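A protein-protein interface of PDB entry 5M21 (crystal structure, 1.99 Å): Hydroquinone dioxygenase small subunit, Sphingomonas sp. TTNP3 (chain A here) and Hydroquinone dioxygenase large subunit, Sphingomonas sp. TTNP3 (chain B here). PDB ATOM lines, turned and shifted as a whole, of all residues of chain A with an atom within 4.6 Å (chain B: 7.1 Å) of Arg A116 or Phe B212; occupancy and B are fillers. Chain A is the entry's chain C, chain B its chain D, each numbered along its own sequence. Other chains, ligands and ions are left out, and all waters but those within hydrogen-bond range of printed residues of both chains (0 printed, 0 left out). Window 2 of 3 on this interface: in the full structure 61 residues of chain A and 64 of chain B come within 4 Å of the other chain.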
ATOM      1  N   LEU A  88      19.424  26.516  27.055  1.00  0.00           N
ATOM      2  CA  LEU A  88      19.955  27.040  25.810  1.00  0.00           C
ATOM      3  C   LEU A  88      18.856  27.762  25.016  1.00  0.00           C
ATOM      4  O   LEU A  88      17.700  27.308  24.932  1.00  0.00           O
ATOM      5  CB  LEU A  88      20.660  25.950  24.962  1.00  0.00           C
ATOM      6  CG  LEU A  88      21.819  25.194  25.669  1.00  0.00           C
ATOM      7  CD1 LEU A  88      22.181  23.908  24.944  1.00  0.00           C
ATOM      8  CD2 LEU A  88      23.023  26.096  25.881  1.00  0.00           C
ATOM      9  N   LEU A  89      19.247  28.895  24.434  1.00  0.00           N
ATOM     10  CA  LEU A  89      18.353  29.734  23.620  1.00  0.00           C
ATOM     11  C   LEU A  89      19.129  30.136  22.339  1.00  0.00           C
ATOM     12  O   LEU A  89      20.240  30.612  22.415  1.00  0.00           O
ATOM     13  CB  LEU A  89      17.936  30.942  24.476  1.00  0.00           C
ATOM     14  CG  LEU A  89      16.905  31.921  23.897  1.00  0.00           C
ATOM     15  CD1 LEU A  89      15.830  32.238  24.913  1.00  0.00           C
ATOM     16  CD2 LEU A  89      17.549  33.198  23.394  1.00  0.00           C
ATOM     17  N   LYS A  90      18.573  29.855  21.171  1.00  0.00           N
ATOM     18  CA  LYS A  90      19.137  30.267  19.877  1.00  0.00           C
ATOM     19  C   LYS A  90      18.832  31.730  19.673  1.00  0.00           C
ATOM     20  O   LYS A  90      17.671  32.059  19.492  1.00  0.00           O
ATOM     21  CB  LYS A  90      18.473  29.464  18.750  1.00  0.00           C
ATOM     22  CG  LYS A  90      19.148  29.660  17.402  1.00  0.00           C
ATOM     23  CD  LYS A  90      20.646  29.398  17.567  1.00  0.00           C
ATOM     24  CE  LYS A  90      21.330  29.165  16.228  1.00  0.00           C
ATOM     25  NZ  LYS A  90      20.920  30.295  15.349  1.00  0.00           N
ATOM     26  N   ASP A  92      18.106  35.257  18.119  1.00  0.00           N
ATOM     27  CA  ASP A  92      17.690  35.873  16.852  1.00  0.00           C
ATOM     28  C   ASP A  92      18.796  36.653  16.147  1.00  0.00           C
ATOM     29  O   ASP A  92      18.993  36.539  14.942  1.00  0.00           O
ATOM     30  CB  ASP A  92      16.516  36.807  17.124  1.00  0.00           C
ATOM     31  CG  ASP A  92      15.195  36.043  17.288  1.00  0.00           C
ATOM     32  OD1 ASP A  92      15.181  34.817  16.974  1.00  0.00           O
ATOM     33  OD2 ASP A  92      14.186  36.660  17.724  1.00  0.00           O
ATOM     34  N   GLY A 115      14.915  35.243  21.221  1.00  0.00           N
ATOM     35  CA  GLY A 115      15.290  34.082  20.408  1.00  0.00           C
ATOM     36  C   GLY A 115      14.438  32.881  20.703  1.00  0.00           C
ATOM     37  O   GLY A 115      13.432  33.017  21.370  1.00  0.00           O
ATOM     38  N   ARG A 116      14.824  31.724  20.186  1.00  0.00           N
ATOM     39  CA  ARG A 116      14.043  30.507  20.326  1.00  0.00           C
ATOM     40  C   ARG A 116      14.658  29.563  21.382  1.00  0.00           C
ATOM     41  O   ARG A 116      15.862  29.337  21.388  1.00  0.00           O
ATOM     42  CB  ARG A 116      13.991  29.785  18.986  1.00  0.00           C
ATOM     43  CG  ARG A 116      13.256  30.579  17.913  1.00  0.00           C
ATOM     44  CD  ARG A 116      13.382  29.925  16.539  1.00  0.00           C
ATOM     45  NE  ARG A 116      14.696  30.251  15.999  1.00  0.00           N
ATOM     46  CZ  ARG A 116      15.382  29.546  15.104  1.00  0.00           C
ATOM     47  NH1 ARG A 116      14.901  28.401  14.600  1.00  0.00           N
ATOM     48  NH2 ARG A 116      16.580  30.009  14.715  1.00  0.00           N
ATOM     49  N   LYS A 117      13.807  29.027  22.258  1.00  0.00           N
ATOM     50  CA  LYS A 117      14.146  27.898  23.132  1.00  0.00           C
ATOM     51  C   LYS A 117      14.835  26.803  22.323  1.00  0.00           C
ATOM     52  O   LYS A 117      14.282  26.242  21.369  1.00  0.00           O
ATOM     53  CB  LYS A 117      12.876  27.346  23.804  1.00  0.00           C
ATOM     54  CG  LYS A 117      13.195  26.390  24.959  1.00  0.00           C
ATOM     55  CD  LYS A 117      11.946  25.712  25.506  1.00  0.00           C
ATOM     56  CE  LYS A 117      12.227  25.034  26.853  1.00  0.00           C
ATOM     57  NZ  LYS A 117      10.990  24.870  27.712  1.00  0.00           N
ATOM     58  N   MET A 118      16.078  26.518  22.703  1.00  0.00           N
ATOM     59  CA  MET A 118      16.879  25.476  22.055  1.00  0.00           C
ATOM     60  C   MET A 118      16.788  24.121  22.773  1.00  0.00           C
ATOM     61  O   MET A 118      16.653  23.060  22.159  1.00  0.00           O
ATOM     62  CB  MET A 118      18.320  25.951  22.080  1.00  0.00           C
ATOM     63  CG  MET A 118      18.994  26.002  20.736  1.00  0.00           C
ATOM     64  SD  MET A 118      20.632  26.766  20.918  1.00  0.00           S
ATOM     65  CE  MET A 118      21.525  25.378  20.258  1.00  0.00           C
ATOM     66  N   ALA B 208      16.387  18.384  23.688  1.00  0.00           N
ATOM     67  CA  ALA B 208      16.464  19.296  22.573  1.00  0.00           C
ATOM     68  C   ALA B 208      15.072  19.628  22.033  1.00  0.00           C
ATOM     69  O   ALA B 208      14.223  18.726  21.849  1.00  0.00           O
ATOM     70  CB  ALA B 208      17.314  18.703  21.461  1.00  0.00           C
ATOM     71  N   GLU B 209      14.858  20.916  21.750  1.00  0.00           N
ATOM     72  CA  GLU B 209      13.660  21.317  21.074  1.00  0.00           C
ATOM     73  C   GLU B 209      13.819  20.862  19.655  1.00  0.00           C
ATOM     74  O   GLU B 209      14.936  20.744  19.197  1.00  0.00           O
ATOM     75  CB  GLU B 209      13.505  22.819  21.156  1.00  0.00           C
ATOM     76  CG  GLU B 209      13.167  23.287  22.560  1.00  0.00           C
ATOM     77  CD  GLU B 209      11.869  22.656  23.041  1.00  0.00           C
ATOM     78  OE1 GLU B 209      10.846  22.790  22.320  1.00  0.00           O
ATOM     79  OE2 GLU B 209      11.872  22.000  24.115  1.00  0.00           O
ATOM     80  N   PRO B 210      12.703  20.611  18.943  1.00  0.00           N
ATOM     81  CA  PRO B 210      12.778  20.172  17.569  1.00  0.00           C
ATOM     82  C   PRO B 210      13.624  21.059  16.680  1.00  0.00           C
ATOM     83  O   PRO B 210      13.478  22.289  16.673  1.00  0.00           O
ATOM     84  CB  PRO B 210      11.313  20.227  17.121  1.00  0.00           C
ATOM     85  CG  PRO B 210      10.573  19.867  18.359  1.00  0.00           C
ATOM     86  CD  PRO B 210      11.295  20.677  19.397  1.00  0.00           C
ATOM     87  N   GLY B 211      14.509  20.420  15.929  1.00  0.00           N
ATOM     88  CA  GLY B 211      15.417  21.128  15.045  1.00  0.00           C
ATOM     89  C   GLY B 211      16.774  21.451  15.636  1.00  0.00           C
ATOM     90  O   GLY B 211      17.686  21.735  14.903  1.00  0.00           O
ATOM     91  N   PHE B 212      16.933  21.401  16.954  1.00  0.00           N
ATOM     92  CA  PHE B 212      18.231  21.763  17.541  1.00  0.00           C
ATOM     93  C   PHE B 212      18.964  20.546  18.091  1.00  0.00           C
ATOM     94  O   PHE B 212      19.841  20.678  18.961  1.00  0.00           O
ATOM     95  CB  PHE B 212      18.037  22.798  18.651  1.00  0.00           C
ATOM     96  CG  PHE B 212      17.417  24.109  18.193  1.00  0.00           C
ATOM     97  CD1 PHE B 212      18.202  25.096  17.556  1.00  0.00           C
ATOM     98  CD2 PHE B 212      16.065  24.387  18.439  1.00  0.00           C
ATOM     99  CE1 PHE B 212      17.639  26.317  17.168  1.00  0.00           C
ATOM    100  CE2 PHE B 212      15.489  25.599  18.025  1.00  0.00           C
ATOM    101  CZ  PHE B 212      16.271  26.566  17.396  1.00  0.00           C
ATOM    102  N   GLU B 213      18.594  19.352  17.637  1.00  0.00           N
ATOM    103  CA  GLU B 213      19.210  18.162  18.239  1.00  0.00           C
ATOM    104  C   GLU B 213      20.707  17.994  18.010  1.00  0.00           C
ATOM    105  O   GLU B 213      21.360  17.382  18.845  1.00  0.00           O
ATOM    106  CB  GLU B 213      18.417  16.841  18.058  1.00  0.00           C
ATOM    107  CG  GLU B 213      17.750  16.579  16.729  1.00  0.00           C
ATOM    108  CD  GLU B 213      16.713  17.615  16.333  1.00  0.00           C
ATOM    109  OE1 GLU B 213      15.586  17.595  16.851  1.00  0.00           O
ATOM    110  OE2 GLU B 213      17.022  18.427  15.461  1.00  0.00           O
ATOM    111  N   ALA B 214      21.268  18.588  16.948  1.00  0.00           N
ATOM    112  CA  ALA B 214      22.716  18.528  16.749  1.00  0.00           C
ATOM    113  C   ALA B 214      23.478  19.550  17.585  1.00  0.00           C
ATOM    114  O   ALA B 214      24.689  19.509  17.653  1.00  0.00           O
ATOM    115  CB  ALA B 214      23.081  18.666  15.264  1.00  0.00           C
ATOM    116  N   GLU B 215      22.812  20.483  18.222  1.00  0.00           N
ATOM    117  CA  GLU B 215      23.580  21.470  19.029  1.00  0.00           C
ATOM    118  C   GLU B 215      23.305  21.447  20.527  1.00  0.00           C
ATOM    119  O   GLU B 215      23.907  22.210  21.303  1.00  0.00           O
ATOM    120  CB  GLU B 215      23.379  22.881  18.477  1.00  0.00           C
ATOM    121  CG  GLU B 215      23.770  22.952  17.013  1.00  0.00           C
ATOM    122  CD  GLU B 215      24.871  23.950  16.770  1.00  0.00           C
ATOM    123  OE1 GLU B 215      26.055  23.560  16.782  1.00  0.00           O
ATOM    124  OE2 GLU B 215      24.543  25.138  16.595  1.00  0.00           O
ATOM    125  N   VAL B 216      22.371  20.597  20.930  1.00  0.00           N
ATOM    126  CA  VAL B 216      22.111  20.394  22.354  1.00  0.00           C
ATOM    127  C   VAL B 216      22.733  19.054  22.651  1.00  0.00           C
ATOM    128  O   VAL B 216      22.209  18.027  22.267  1.00  0.00           O
ATOM    129  CB  VAL B 216      20.593  20.404  22.684  1.00  0.00           C
ATOM    130  CG1 VAL B 216      20.388  20.458  24.185  1.00  0.00           C
ATOM    131  CG2 VAL B 216      19.866  21.592  21.995  1.00  0.00           C
ATOM    132  N   SER B 217      23.871  19.066  23.299  1.00  0.00           N
ATOM    133  CA  SER B 217      24.644  17.845  23.473  1.00  0.00           C
ATOM    134  C   SER B 217      25.416  17.820  24.825  1.00  0.00           C
ATOM    135  O   SER B 217      25.978  18.840  25.272  1.00  0.00           O
ATOM    136  CB  SER B 217      25.609  17.671  22.273  1.00  0.00           C
ATOM    137  OG  SER B 217      26.349  16.474  22.317  1.00  0.00           O
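The backbone NH (N) of Glu B209 is in hydrogen-bond range of the backbone carbonyl oxygen (O) of Met A118, 2.8 Å away.
N of Lys A90 lies within hydrogen-bond range of O of Arg A116, at 2.8 Å. The backbone NH (N) of Met A118 sits at hydrogen-bond distance from the backbone carbonyl oxygen (O) of Leu A88 (2.9 Å). N of Lys A90 is in hydrogen-bond range of SD of Met A118, 3.7 Å away.
Among the printed residues, pairs that only touch across the chains: Leu A88 with Val B216 (3.96 Å), Lys A90 with Phe B212 (3.6 Å), Arg A116 with Phe B212 (3.6 Å), Lys A117 with Glu B209 (3.4 Å), Lys A117 with Phe B212 (3.6 Å), Met A118 with Ala B208 (3.8 Å), Met A118 with Phe B212 (3.4 Å), Met A118 with Glu B215 (3.6 Å) and Met A118 with Val B216 (3.5 Å).
Arg A116 touches just one residue of chain B: Phe B212 (3.6 Å). Of the printed residues of chain B, Met A118 touches Ala B208, Glu B209, Phe B212, Glu B215 and Val B216. Printed residues of chain A within 4 Å of Ala B208: Met A118 (3.8 Å). Pro B210 touches none of the printed residues of chain A. Of chain A, only Lys A90 (3.6 Å), Arg A116 (3.6 Å), Lys A117 (3.6 Å) and Met A118 (3.4 Å) come within 4 Å of Phe B212. Ala B214 touches none of the printed residues of chain A. The nearest residue of chain B that does not touch Arg A116 is Glu B209 (6.6 Å).
Of the 8 printed residues of chain A, 5 touch a printed residue of chain B. Printed residues of chain A that touch a printed residue of chain B: Leu A88, Lys A90, Arg A116, Lys A117 and Met A118. Among the printed residues, no Asp or Glu carboxylate lies within 4 Å of a Lys or Arg side-chain nitrogen of the other chain.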
